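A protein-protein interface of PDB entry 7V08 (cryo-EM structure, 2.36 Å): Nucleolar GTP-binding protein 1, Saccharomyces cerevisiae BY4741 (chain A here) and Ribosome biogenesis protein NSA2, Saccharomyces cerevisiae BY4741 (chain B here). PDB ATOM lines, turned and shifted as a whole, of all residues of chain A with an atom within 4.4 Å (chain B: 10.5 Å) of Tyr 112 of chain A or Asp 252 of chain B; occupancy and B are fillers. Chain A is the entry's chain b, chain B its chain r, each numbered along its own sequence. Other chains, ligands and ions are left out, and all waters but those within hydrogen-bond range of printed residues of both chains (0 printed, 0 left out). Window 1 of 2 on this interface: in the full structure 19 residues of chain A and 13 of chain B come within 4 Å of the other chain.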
ATOM      1  N   VAL A 108      16.594   9.108   2.190  1.00  0.00           N
ATOM      2  CA  VAL A 108      17.230  10.420   2.049  1.00  0.00           C
ATOM      3  C   VAL A 108      18.070  10.482   0.777  1.00  0.00           C
ATOM      4  O   VAL A 108      18.000  11.460   0.015  1.00  0.00           O
ATOM      5  CB  VAL A 108      18.074  10.745   3.298  1.00  0.00           C
ATOM      6  CG1 VAL A 108      19.001  11.929   3.041  1.00  0.00           C
ATOM      7  CG2 VAL A 108      17.179  11.035   4.489  1.00  0.00           C
ATOM      8  N   ALA A 109      18.864   9.437   0.521  1.00  0.00           N
ATOM      9  CA  ALA A 109      19.683   9.421  -0.691  1.00  0.00           C
ATOM     10  C   ALA A 109      18.821   9.491  -1.947  1.00  0.00           C
ATOM     11  O   ALA A 109      19.106  10.279  -2.862  1.00  0.00           O
ATOM     12  CB  ALA A 109      20.570   8.180  -0.719  1.00  0.00           C
ATOM     13  N   ARG A 110      17.740   8.698  -1.995  1.00  0.00           N
ATOM     14  CA  ARG A 110      16.877   8.703  -3.175  1.00  0.00           C
ATOM     15  C   ARG A 110      16.216  10.065  -3.385  1.00  0.00           C
ATOM     16  O   ARG A 110      16.196  10.595  -4.507  1.00  0.00           O
ATOM     17  CB  ARG A 110      15.818   7.604  -3.060  1.00  0.00           C
ATOM     18  CG  ARG A 110      16.353   6.199  -3.226  1.00  0.00           C
ATOM     19  CD  ARG A 110      15.229   5.212  -3.488  1.00  0.00           C
ATOM     20  NE  ARG A 110      14.202   5.240  -2.455  1.00  0.00           N
ATOM     21  CZ  ARG A 110      14.147   4.401  -1.432  1.00  0.00           C
ATOM     22  NH1 ARG A 110      15.060   3.460  -1.260  1.00  0.00           N
ATOM     23  NH2 ARG A 110      13.149   4.506  -0.559  1.00  0.00           N
ATOM     24  N   ASP A 111      15.693  10.657  -2.305  1.00  0.00           N
ATOM     25  CA  ASP A 111      15.032  11.954  -2.407  1.00  0.00           C
ATOM     26  C   ASP A 111      15.978  13.020  -2.932  1.00  0.00           C
ATOM     27  O   ASP A 111      15.618  13.796  -3.827  1.00  0.00           O
ATOM     28  CB  ASP A 111      14.482  12.379  -1.048  1.00  0.00           C
ATOM     29  CG  ASP A 111      13.327  11.527  -0.595  1.00  0.00           C
ATOM     30  OD1 ASP A 111      12.821  10.725  -1.407  1.00  0.00           O
ATOM     31  OD2 ASP A 111      12.926  11.648   0.578  1.00  0.00           O
ATOM     32  N   TYR A 112      17.197  13.079  -2.399  1.00  0.00           N
ATOM     33  CA  TYR A 112      18.049  14.187  -2.800  1.00  0.00           C
ATOM     34  C   TYR A 112      18.690  13.968  -4.159  1.00  0.00           C
ATOM     35  O   TYR A 112      18.978  14.948  -4.843  1.00  0.00           O
ATOM     36  CB  TYR A 112      19.086  14.477  -1.724  1.00  0.00           C
ATOM     37  CG  TYR A 112      18.491  15.336  -0.641  1.00  0.00           C
ATOM     38  CD1 TYR A 112      17.720  14.775   0.365  1.00  0.00           C
ATOM     39  CD2 TYR A 112      18.642  16.712  -0.661  1.00  0.00           C
ATOM     40  CE1 TYR A 112      17.145  15.554   1.337  1.00  0.00           C
ATOM     41  CE2 TYR A 112      18.066  17.502   0.307  1.00  0.00           C
ATOM     42  CZ  TYR A 112      17.324  16.917   1.307  1.00  0.00           C
ATOM     43  OH  TYR A 112      16.758  17.699   2.280  1.00  0.00           O
ATOM     44  N   VAL A 113      18.885  12.722  -4.600  1.00  0.00           N
ATOM     45  CA  VAL A 113      19.285  12.520  -5.992  1.00  0.00           C
ATOM     46  C   VAL A 113      18.184  13.002  -6.937  1.00  0.00           C
ATOM     47  O   VAL A 113      18.447  13.720  -7.925  1.00  0.00           O
ATOM     48  CB  VAL A 113      19.656  11.046  -6.241  1.00  0.00           C
ATOM     49  CG1 VAL A 113      19.774  10.773  -7.720  1.00  0.00           C
ATOM     50  CG2 VAL A 113      20.962  10.715  -5.557  1.00  0.00           C
ATOM     51  N   ARG A 114      16.927  12.655  -6.625  1.00  0.00           N
ATOM     52  CA  ARG A 114      15.814  13.120  -7.445  1.00  0.00           C
ATOM     53  C   ARG A 114      15.737  14.645  -7.475  1.00  0.00           C
ATOM     54  O   ARG A 114      15.484  15.235  -8.528  1.00  0.00           O
ATOM     55  CB  ARG A 114      14.502  12.527  -6.939  1.00  0.00           C
ATOM     56  CG  ARG A 114      13.361  12.655  -7.921  1.00  0.00           C
ATOM     57  CD  ARG A 114      12.077  12.015  -7.410  1.00  0.00           C
ATOM     58  NE  ARG A 114      12.297  10.680  -6.870  1.00  0.00           N
ATOM     59  CZ  ARG A 114      12.147  10.354  -5.594  1.00  0.00           C
ATOM     60  NH1 ARG A 114      11.736  11.237  -4.700  1.00  0.00           N
ATOM     61  NH2 ARG A 114      12.415   9.111  -5.207  1.00  0.00           N
ATOM     62  N   LEU A 115      15.949  15.300  -6.330  1.00  0.00           N
ATOM     63  CA  LEU A 115      15.977  16.763  -6.317  1.00  0.00           C
ATOM     64  C   LEU A 115      17.144  17.313  -7.122  1.00  0.00           C
ATOM     65  O   LEU A 115      16.977  18.277  -7.875  1.00  0.00           O
ATOM     66  CB  LEU A 115      16.055  17.297  -4.892  1.00  0.00           C
ATOM     67  CG  LEU A 115      14.836  17.118  -3.997  1.00  0.00           C
ATOM     68  CD1 LEU A 115      15.054  17.912  -2.747  1.00  0.00           C
ATOM     69  CD2 LEU A 115      13.571  17.552  -4.704  1.00  0.00           C
ATOM     70  N   LEU A 116      18.329  16.718  -6.972  1.00  0.00           N
ATOM     71  CA  LEU A 116      19.528  17.200  -7.641  1.00  0.00           C
ATOM     72  C   LEU A 116      19.407  17.142  -9.148  1.00  0.00           C
ATOM     73  O   LEU A 116      20.135  17.856  -9.837  1.00  0.00           O
ATOM     74  CB  LEU A 116      20.746  16.385  -7.210  1.00  0.00           C
ATOM     75  CG  LEU A 116      21.602  16.955  -6.087  1.00  0.00           C
ATOM     76  CD1 LEU A 116      22.601  15.930  -5.575  1.00  0.00           C
ATOM     77  CD2 LEU A 116      22.318  18.187  -6.580  1.00  0.00           C
ATOM     78  N   LEU A 128      22.090  21.242  -1.779  1.00  0.00           N
ATOM     79  CA  LEU A 128      21.299  20.017  -1.715  1.00  0.00           C
ATOM     80  C   LEU A 128      22.134  18.830  -1.237  1.00  0.00           C
ATOM     81  O   LEU A 128      21.666  18.023  -0.424  1.00  0.00           O
ATOM     82  CB  LEU A 128      20.671  19.729  -3.076  1.00  0.00           C
ATOM     83  CG  LEU A 128      19.431  20.571  -3.398  1.00  0.00           C
ATOM     84  CD1 LEU A 128      19.043  20.449  -4.855  1.00  0.00           C
ATOM     85  CD2 LEU A 128      18.258  20.180  -2.513  1.00  0.00           C
ATOM     86  N   ALA A 131      22.696  19.212   2.427  1.00  0.00           N
ATOM     87  CA  ALA A 131      21.478  18.873   3.153  1.00  0.00           C
ATOM     88  C   ALA A 131      21.306  17.365   3.275  1.00  0.00           C
ATOM     89  O   ALA A 131      20.964  16.862   4.351  1.00  0.00           O
ATOM     90  CB  ALA A 131      20.262  19.496   2.477  1.00  0.00           C
ATOM     91  N   ALA A 132      21.555  16.627   2.189  1.00  0.00           N
ATOM     92  CA  ALA A 132      21.424  15.171   2.228  1.00  0.00           C
ATOM     93  C   ALA A 132      22.398  14.548   3.223  1.00  0.00           C
ATOM     94  O   ALA A 132      22.009  13.722   4.062  1.00  0.00           O
ATOM     95  CB  ALA A 132      21.645  14.588   0.835  1.00  0.00           C
ATOM     96  N   ARG A 135      21.363  15.359   6.845  1.00  0.00           N
ATOM     97  CA  ARG A 135      20.255  14.526   7.303  1.00  0.00           C
ATOM     98  C   ARG A 135      20.712  13.106   7.618  1.00  0.00           C
ATOM     99  O   ARG A 135      20.287  12.521   8.625  1.00  0.00           O
ATOM    100  CB  ARG A 135      19.139  14.536   6.263  1.00  0.00           C
ATOM    101  CG  ARG A 135      18.473  15.901   6.131  1.00  0.00           C
ATOM    102  CD  ARG A 135      17.441  15.936   5.025  1.00  0.00           C
ATOM    103  NE  ARG A 135      16.241  15.192   5.381  1.00  0.00           N
ATOM    104  CZ  ARG A 135      15.012  15.681   5.330  1.00  0.00           C
ATOM    105  NH1 ARG A 135      14.771  16.900   4.882  1.00  0.00           N
ATOM    106  NH2 ARG A 135      13.997  14.926   5.733  1.00  0.00           N
ATOM    107  N   THR B 152      11.422  26.159 -11.650  1.00  0.00           N
ATOM    108  CA  THR B 152      12.584  25.597 -10.974  1.00  0.00           C
ATOM    109  C   THR B 152      12.433  25.535  -9.462  1.00  0.00           C
ATOM    110  O   THR B 152      13.298  24.960  -8.797  1.00  0.00           O
ATOM    111  CB  THR B 152      13.836  26.409 -11.313  1.00  0.00           C
ATOM    112  OG1 THR B 152      13.727  27.712 -10.731  1.00  0.00           O
ATOM    113  CG2 THR B 152      13.978  26.555 -12.811  1.00  0.00           C
ATOM    114  N   LYS B 153      11.369  26.103  -8.906  1.00  0.00           N
ATOM    115  CA  LYS B 153      11.137  26.126  -7.469  1.00  0.00           C
ATOM    116  C   LYS B 153      10.136  25.048  -7.073  1.00  0.00           C
ATOM    117  O   LYS B 153       9.568  24.350  -7.914  1.00  0.00           O
ATOM    118  CB  LYS B 153      10.633  27.500  -7.021  1.00  0.00           C
ATOM    119  CG  LYS B 153      11.529  28.654  -7.396  1.00  0.00           C
ATOM    120  CD  LYS B 153      12.956  28.423  -6.946  1.00  0.00           C
ATOM    121  CE  LYS B 153      13.749  29.709  -6.981  1.00  0.00           C
ATOM    122  NZ  LYS B 153      13.411  30.526  -8.172  1.00  0.00           N
ATOM    123  N   HIS B 154       9.935  24.911  -5.764  1.00  0.00           N
ATOM    124  CA  HIS B 154       8.983  23.948  -5.233  1.00  0.00           C
ATOM    125  C   HIS B 154       7.568  24.509  -5.278  1.00  0.00           C
ATOM    126  O   HIS B 154       7.355  25.708  -5.091  1.00  0.00           O
ATOM    127  CB  HIS B 154       9.353  23.562  -3.801  1.00  0.00           C
ATOM    128  CG  HIS B 154      10.521  22.634  -3.717  1.00  0.00           C
ATOM    129  ND1 HIS B 154      10.395  21.313  -3.356  1.00  0.00           N
ATOM    130  CD2 HIS B 154      11.836  22.832  -3.965  1.00  0.00           C
ATOM    131  CE1 HIS B 154      11.583  20.739  -3.375  1.00  0.00           C
ATOM    132  NE2 HIS B 154      12.474  21.638  -3.745  1.00  0.00           N
ATOM    133  N   ALA B 176       8.601  15.797  -8.846  1.00  0.00           N
ATOM    134  CA  ALA B 176       9.600  15.737  -7.787  1.00  0.00           C
ATOM    135  C   ALA B 176       9.679  17.031  -6.989  1.00  0.00           C
ATOM    136  O   ALA B 176      10.080  17.003  -5.824  1.00  0.00           O
ATOM    137  CB  ALA B 176      10.975  15.405  -8.369  1.00  0.00           C
ATOM    138  N   LEU B 177       9.301  18.159  -7.577  1.00  0.00           N
ATOM    139  CA  LEU B 177       9.364  19.434  -6.881  1.00  0.00           C
ATOM    140  C   LEU B 177       8.042  19.823  -6.234  1.00  0.00           C
ATOM    141  O   LEU B 177       7.944  20.915  -5.677  1.00  0.00           O
ATOM    142  CB  LEU B 177       9.841  20.535  -7.835  1.00  0.00           C
ATOM    143  CG  LEU B 177      11.213  20.287  -8.476  1.00  0.00           C
ATOM    144  CD1 LEU B 177      11.602  21.384  -9.450  1.00  0.00           C
ATOM    145  CD2 LEU B 177      12.279  20.116  -7.408  1.00  0.00           C
ATOM    146  N   GLN B 179       5.327  19.628  -3.280  1.00  0.00           N
ATOM    147  CA  GLN B 179       5.330  19.365  -1.847  1.00  0.00           C
ATOM    148  C   GLN B 179       3.905  19.294  -1.320  1.00  0.00           C
ATOM    149  O   GLN B 179       3.008  19.971  -1.823  1.00  0.00           O
ATOM    150  CB  GLN B 179       6.084  20.452  -1.063  1.00  0.00           C
ATOM    151  CG  GLN B 179       7.535  20.675  -1.459  1.00  0.00           C
ATOM    152  CD  GLN B 179       8.493  19.750  -0.742  1.00  0.00           C
ATOM    153  OE1 GLN B 179       8.135  18.644  -0.357  1.00  0.00           O
ATOM    154  NE2 GLN B 179       9.725  20.207  -0.555  1.00  0.00           N
ATOM    155  N   LYS B 181       3.569  18.744   2.527  1.00  0.00           N
ATOM    156  CA  LYS B 181       3.646  18.925   3.970  1.00  0.00           C
ATOM    157  C   LYS B 181       4.815  19.839   4.312  1.00  0.00           C
ATOM    158  O   LYS B 181       5.759  19.995   3.537  1.00  0.00           O
ATOM    159  CB  LYS B 181       3.772  17.571   4.684  1.00  0.00           C
ATOM    160  CG  LYS B 181       2.541  16.685   4.532  1.00  0.00           C
ATOM    161  CD  LYS B 181       2.744  15.288   5.078  1.00  0.00           C
ATOM    162  CE  LYS B 181       2.806  15.279   6.591  1.00  0.00           C
ATOM    163  NZ  LYS B 181       1.599  15.875   7.213  1.00  0.00           N
ATOM    164  N   ASN B 183       7.216  21.669   7.807  1.00  0.00           N
ATOM    165  CA  ASN B 183       7.580  21.690   9.221  1.00  0.00           C
ATOM    166  C   ASN B 183       7.175  23.043   9.791  1.00  0.00           C
ATOM    167  O   ASN B 183       7.812  24.055   9.494  1.00  0.00           O
ATOM    168  CB  ASN B 183       9.078  21.461   9.414  1.00  0.00           C
ATOM    169  CG  ASN B 183       9.549  20.135   8.866  1.00  0.00           C
ATOM    170  OD1 ASN B 183       9.264  19.087   9.426  1.00  0.00           O
ATOM    171  ND2 ASN B 183      10.296  20.179   7.775  1.00  0.00           N
ATOM    172  N   PHE B 194       4.956  18.292  11.676  1.00  0.00           N
ATOM    173  CA  PHE B 194       4.888  18.087  10.232  1.00  0.00           C
ATOM    174  C   PHE B 194       3.424  18.121   9.796  1.00  0.00           C
ATOM    175  O   PHE B 194       2.698  17.139   9.964  1.00  0.00           O
ATOM    176  CB  PHE B 194       5.552  16.762   9.858  1.00  0.00           C
ATOM    177  CG  PHE B 194       6.052  16.699   8.439  1.00  0.00           C
ATOM    178  CD1 PHE B 194       6.476  17.836   7.783  1.00  0.00           C
ATOM    179  CD2 PHE B 194       6.108  15.490   7.770  1.00  0.00           C
ATOM    180  CE1 PHE B 194       6.941  17.773   6.482  1.00  0.00           C
ATOM    181  CE2 PHE B 194       6.567  15.419   6.471  1.00  0.00           C
ATOM    182  CZ  PHE B 194       6.985  16.561   5.826  1.00  0.00           C
ATOM    183  N   LEU B 215       6.298  27.895  -3.840  1.00  0.00           N
ATOM    184  CA  LEU B 215       6.684  27.950  -2.431  1.00  0.00           C
ATOM    185  C   LEU B 215       8.137  28.416  -2.343  1.00  0.00           C
ATOM    186  O   LEU B 215       9.067  27.621  -2.451  1.00  0.00           O
ATOM    187  CB  LEU B 215       6.499  26.592  -1.771  1.00  0.00           C
ATOM    188  CG  LEU B 215       5.107  25.969  -1.840  1.00  0.00           C
ATOM    189  CD1 LEU B 215       5.190  24.475  -1.660  1.00  0.00           C
ATOM    190  CD2 LEU B 215       4.216  26.566  -0.782  1.00  0.00           C
ATOM    191  N   THR B 216       8.327  29.710  -2.143  1.00  0.00           N
ATOM    192  CA  THR B 216       9.641  30.273  -1.876  1.00  0.00           C
ATOM    193  C   THR B 216       9.624  30.930  -0.503  1.00  0.00           C
ATOM    194  O   THR B 216       8.621  30.900   0.210  1.00  0.00           O
ATOM    195  CB  THR B 216      10.058  31.272  -2.961  1.00  0.00           C
ATOM    196  OG1 THR B 216       9.037  32.259  -3.135  1.00  0.00           O
ATOM    197  CG2 THR B 216      10.310  30.561  -4.278  1.00  0.00           C
ATOM    198  N   LYS B 217      10.756  31.516  -0.135  1.00  0.00           N
ATOM    199  CA  LYS B 217      10.890  32.140   1.170  1.00  0.00           C
ATOM    200  C   LYS B 217       9.925  33.309   1.319  1.00  0.00           C
ATOM    201  O   LYS B 217       9.820  34.168   0.440  1.00  0.00           O
ATOM    202  CB  LYS B 217      12.326  32.614   1.375  1.00  0.00           C
ATOM    203  CG  LYS B 217      12.588  33.132   2.757  1.00  0.00           C
ATOM    204  CD  LYS B 217      14.065  33.278   3.028  1.00  0.00           C
ATOM    205  CE  LYS B 217      14.295  34.277   4.132  1.00  0.00           C
ATOM    206  NZ  LYS B 217      15.689  34.223   4.644  1.00  0.00           N
ATOM    207  N   VAL B 245       6.602  30.785   5.190  1.00  0.00           N
ATOM    208  CA  VAL B 245       7.776  29.993   4.841  1.00  0.00           C
ATOM    209  C   VAL B 245       9.031  30.784   5.182  1.00  0.00           C
ATOM    210  O   VAL B 245       9.165  31.954   4.806  1.00  0.00           O
ATOM    211  CB  VAL B 245       7.738  29.604   3.353  1.00  0.00           C
ATOM    212  CG1 VAL B 245       8.998  28.852   2.956  1.00  0.00           C
ATOM    213  CG2 VAL B 245       6.503  28.772   3.046  1.00  0.00           C
ATOM    214  N   THR B 246       9.953  30.150   5.898  1.00  0.00           N
ATOM    215  CA  THR B 246      11.121  30.818   6.455  1.00  0.00           C
ATOM    216  C   THR B 246      12.440  30.362   5.844  1.00  0.00           C
ATOM    217  O   THR B 246      13.488  30.888   6.220  1.00  0.00           O
ATOM    218  CB  THR B 246      11.169  30.611   7.974  1.00  0.00           C
ATOM    219  OG1 THR B 246      11.196  29.209   8.268  1.00  0.00           O
ATOM    220  CG2 THR B 246       9.966  31.234   8.643  1.00  0.00           C
ATOM    221  N   ASN B 247      12.424  29.432   4.893  1.00  0.00           N
ATOM    222  CA  ASN B 247      13.652  28.929   4.294  1.00  0.00           C
ATOM    223  C   ASN B 247      13.522  28.934   2.774  1.00  0.00           C
ATOM    224  O   ASN B 247      12.554  29.450   2.213  1.00  0.00           O
ATOM    225  CB  ASN B 247      13.984  27.527   4.817  1.00  0.00           C
ATOM    226  CG  ASN B 247      13.027  26.469   4.316  1.00  0.00           C
ATOM    227  OD1 ASN B 247      11.828  26.701   4.202  1.00  0.00           O
ATOM    228  ND2 ASN B 247      13.555  25.295   4.018  1.00  0.00           N
ATOM    229  N   GLU B 248      14.516  28.354   2.105  1.00  0.00           N
ATOM    230  CA  GLU B 248      14.475  28.173   0.659  1.00  0.00           C
ATOM    231  C   GLU B 248      14.406  26.685   0.338  1.00  0.00           C
ATOM    232  O   GLU B 248      15.438  25.985   0.358  1.00  0.00           O
ATOM    233  CB  GLU B 248      15.684  28.826  -0.013  1.00  0.00           C
ATOM    234  CG  GLU B 248      15.825  30.326   0.264  1.00  0.00           C
ATOM    235  CD  GLU B 248      14.951  31.211  -0.625  1.00  0.00           C
ATOM    236  OE1 GLU B 248      13.896  30.752  -1.121  1.00  0.00           O
ATOM    237  OE2 GLU B 248      15.326  32.384  -0.831  1.00  0.00           O
ATOM    238  N   PRO B 249      13.210  26.155   0.069  1.00  0.00           N
ATOM    239  CA  PRO B 249      13.083  24.718  -0.211  1.00  0.00           C
ATOM    240  C   PRO B 249      13.827  24.262  -1.451  1.00  0.00           C
ATOM    241  O   PRO B 249      14.207  23.091  -1.521  1.00  0.00           O
ATOM    242  CB  PRO B 249      11.567  24.513  -0.341  1.00  0.00           C
ATOM    243  CG  PRO B 249      10.968  25.848  -0.384  1.00  0.00           C
ATOM    244  CD  PRO B 249      11.905  26.819   0.210  1.00  0.00           C
ATOM    245  N   ASP B 250      14.073  25.137  -2.423  1.00  0.00           N
ATOM    246  CA  ASP B 250      14.900  24.733  -3.551  1.00  0.00           C
ATOM    247  C   ASP B 250      16.346  24.484  -3.138  1.00  0.00           C
ATOM    248  O   ASP B 250      17.052  23.736  -3.819  1.00  0.00           O
ATOM    249  CB  ASP B 250      14.838  25.780  -4.663  1.00  0.00           C
ATOM    250  CG  ASP B 250      15.271  27.151  -4.199  1.00  0.00           C
ATOM    251  OD1 ASP B 250      14.588  27.742  -3.334  1.00  0.00           O
ATOM    252  OD2 ASP B 250      16.307  27.635  -4.697  1.00  0.00           O
ATOM    253  N   ARG B 251      16.795  25.072  -2.034  1.00  0.00           N
ATOM    254  CA  ARG B 251      18.155  24.853  -1.567  1.00  0.00           C
ATOM    255  C   ARG B 251      18.264  23.733  -0.545  1.00  0.00           C
ATOM    256  O   ARG B 251      19.276  23.032  -0.516  1.00  0.00           O
ATOM    257  CB  ARG B 251      18.728  26.129  -0.957  1.00  0.00           C
ATOM    258  CG  ARG B 251      18.913  27.260  -1.918  1.00  0.00           C
ATOM    259  CD  ARG B 251      19.496  28.427  -1.180  1.00  0.00           C
ATOM    260  NE  ARG B 251      19.240  29.693  -1.847  1.00  0.00           N
ATOM    261  CZ  ARG B 251      19.450  30.877  -1.295  1.00  0.00           C
ATOM    262  NH1 ARG B 251      19.896  30.991  -0.056  1.00  0.00           N
ATOM    263  NH2 ARG B 251      19.206  31.973  -2.006  1.00  0.00           N
ATOM    264  N   ASP B 252      17.279  23.554   0.332  1.00  0.00           N
ATOM    265  CA  ASP B 252      17.447  22.527   1.354  1.00  0.00           C
ATOM    266  C   ASP B 252      16.473  21.363   1.252  1.00  0.00           C
ATOM    267  O   ASP B 252      16.508  20.482   2.115  1.00  0.00           O
ATOM    268  CB  ASP B 252      17.379  23.139   2.754  1.00  0.00           C
ATOM    269  CG  ASP B 252      16.068  23.797   3.029  1.00  0.00           C
ATOM    270  OD1 ASP B 252      15.237  23.845   2.105  1.00  0.00           O
ATOM    271  OD2 ASP B 252      15.873  24.269   4.167  1.00  0.00           O
ATOM    272  N   GLY B 253      15.619  21.320   0.237  1.00  0.00           N
ATOM    273  CA  GLY B 253      14.794  20.158  -0.020  1.00  0.00           C
ATOM    274  C   GLY B 253      13.592  19.966   0.875  1.00  0.00           C
ATOM    275  O   GLY B 253      12.961  18.908   0.809  1.00  0.00           O
ATOM    276  N   CYS B 254      13.248  20.946   1.704  1.00  0.00           N
ATOM    277  CA  CYS B 254      12.123  20.818   2.617  1.00  0.00           C
ATOM    278  C   CYS B 254      11.514  22.190   2.836  1.00  0.00           C
ATOM    279  O   CYS B 254      12.144  23.214   2.573  1.00  0.00           O
ATOM    280  CB  CYS B 254      12.543  20.199   3.960  1.00  0.00           C
ATOM    281  SG  CYS B 254      13.898  21.054   4.811  1.00  0.00           S
ATOM    282  N   VAL B 255      10.286  22.202   3.339  1.00  0.00           N
ATOM    283  CA  VAL B 255       9.555  23.435   3.608  1.00  0.00           C
ATOM    284  C   VAL B 255       9.534  23.657   5.115  1.00  0.00           C
ATOM    285  O   VAL B 255       9.061  22.801   5.872  1.00  0.00           O
ATOM    286  CB  VAL B 255       8.131  23.395   3.031  1.00  0.00           C
ATOM    287  CG1 VAL B 255       7.496  24.785   3.069  1.00  0.00           C
ATOM    288  CG2 VAL B 255       8.136  22.848   1.608  1.00  0.00           C
ATOM    289  N   ASN B 256      10.059  24.795   5.546  1.00  0.00           N
ATOM    290  CA  ASN B 256      10.006  25.225   6.935  1.00  0.00           C
ATOM    291  C   ASN B 256       9.114  26.455   7.017  1.00  0.00           C
ATOM    292  O   ASN B 256       9.278  27.386   6.230  1.00  0.00           O
ATOM    293  CB  ASN B 256      11.404  25.547   7.471  1.00  0.00           C
ATOM    294  CG  ASN B 256      12.297  24.332   7.566  1.00  0.00           C
ATOM    295  OD1 ASN B 256      11.836  23.238   7.850  1.00  0.00           O
ATOM    296  ND2 ASN B 256      13.589  24.529   7.353  1.00  0.00           N
ATOM    297  N   ALA B 257       8.174  26.463   7.958  1.00  0.00           N
ATOM    298  CA  ALA B 257       7.304  27.613   8.147  1.00  0.00           C
ATOM    299  C   ALA B 257       7.071  27.859   9.631  1.00  0.00           C
ATOM    300  O   ALA B 257       7.070  26.937  10.447  1.00  0.00           O
ATOM    301  CB  ALA B 257       5.967  27.431   7.416  1.00  0.00           C
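The side-chain hydroxyl (OH) of Tyr 112 of chain A is in hydrogen-bond range of the backbone carbonyl oxygen (O) of Asp 252 of chain B, 2.8 Å away.
The guanidinium group (NH1) of Arg 114 of chain A lies within salt-bridge range of the side-chain carboxylate (OD1) of Asp 111 of chain A (3.5 Å). The side-chain hydroxyl (OH) of Tyr 112 of chain A sits close to the guanidinium group (NH1) of Arg 135 of chain A (3.4 Å). ND1 of His 154 of chain B lies within hydrogen-bond range of NE2 of Gln 179 of chain B (3.1 Å). O of His 154 of chain B is in hydrogen-bond range of N of Leu 215 of chain B (2.7 Å). A ring nitrogen (NE2) of His 154 of chain B sits at hydrogen-bond distance from the backbone carbonyl oxygen (O) of Pro 249 of chain B, 3.2 Å away. The backbone carbonyl oxygen (O) of Asp 252 of chain B is in hydrogen-bond range of the side-chain sulfur (SG) of Cys 254 of chain B (3.8 Å).
OH of Tyr 112 of chain A touches CA of Gly 253 of chain B (3.9 Å). CG of Arg 114 of chain A touches CB of Ala 176 of chain B, 3.7 Å away. CE1 of His 154 of chain B touches CD2 of Leu 115 of chain A, at 3.98 Å. Leu 115 of chain A touches Ala 176 of chain B (CD2 to O, 3.7 Å). Leu 115 of chain A touches Leu 177 of chain B (CD2 to CD2, 3.9 Å). Leu 115 of chain A touches Gly 253 of chain B (CD1 to CA, 3.5 Å). CD2 of Leu 128 of chain A touches O of Asp 250 of chain B, at 3.98 Å. Arg 251 of chain B touches Leu 128 of chain A. N of Gly 253 of chain B touches CD2 of Leu 128 of chain A (3.98 Å). CB of Ala 131 of chain A touches O of Asp 252 of chain B, at 3.9 Å.
Of the printed residues of chain B, Tyr 112 of chain A touches Asp 252 and Gly 253. Asp 252 of chain B touches just these residues of chain A: Tyr 112 and Ala 131. No residue of chain B comes within 4 Å of Val 108 of chain A. No residue of chain B comes within 4 Å of Asp 111 of chain A. No residue of chain B comes within 4 Å of Val 113 of chain A. No residue of chain B comes within 4 Å of Leu 116 of chain A. Of chain B, only Asp 250, Arg 251 and Gly 253 come within 4 Å of Leu 128 of chain A. Ala 131 of chain A touches one residue of chain B. No residue of chain B comes within 4 Å of Ala 132 of chain A. Of the printed residues of chain A, Arg 251 of chain B touches Leu 128. Of the printed residues of chain A, Asp 250 of chain B touches Leu 128. Printed residues of chain A within 4 Å of Gly 253 of chain B: Tyr 112, Leu 115 and Leu 128. Printed residues of chain A within 4 Å of Leu 177 of chain B: Leu 115. Gln 179 of chain B touches none of the printed residues of chain A. Thr 216 of chain B touches none of the printed residues of chain A. The nearest residue of chain A that does not touch Asp 252 of chain B is Leu 128 of chain A (4.3 Å). The nearest printed residue of chain B that does not touch Arg 114 of chain A is Leu 177 of chain B (5.9 Å).
Hydrophobic or aromatic side chains of chain A that line the printed part of chain B: Tyr 112, Leu 115, Leu 128 and Ala 131. Along chain A the printed residues that touch a printed residue of chain B span positions 112 to 131. Of the 25 printed residues of chain B, 7 touch a printed residue of chain A. Among the printed residues, no Asp or Glu carboxylate lies within 4 Å of a Lys or Arg side-chain nitrogen of the other chain.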
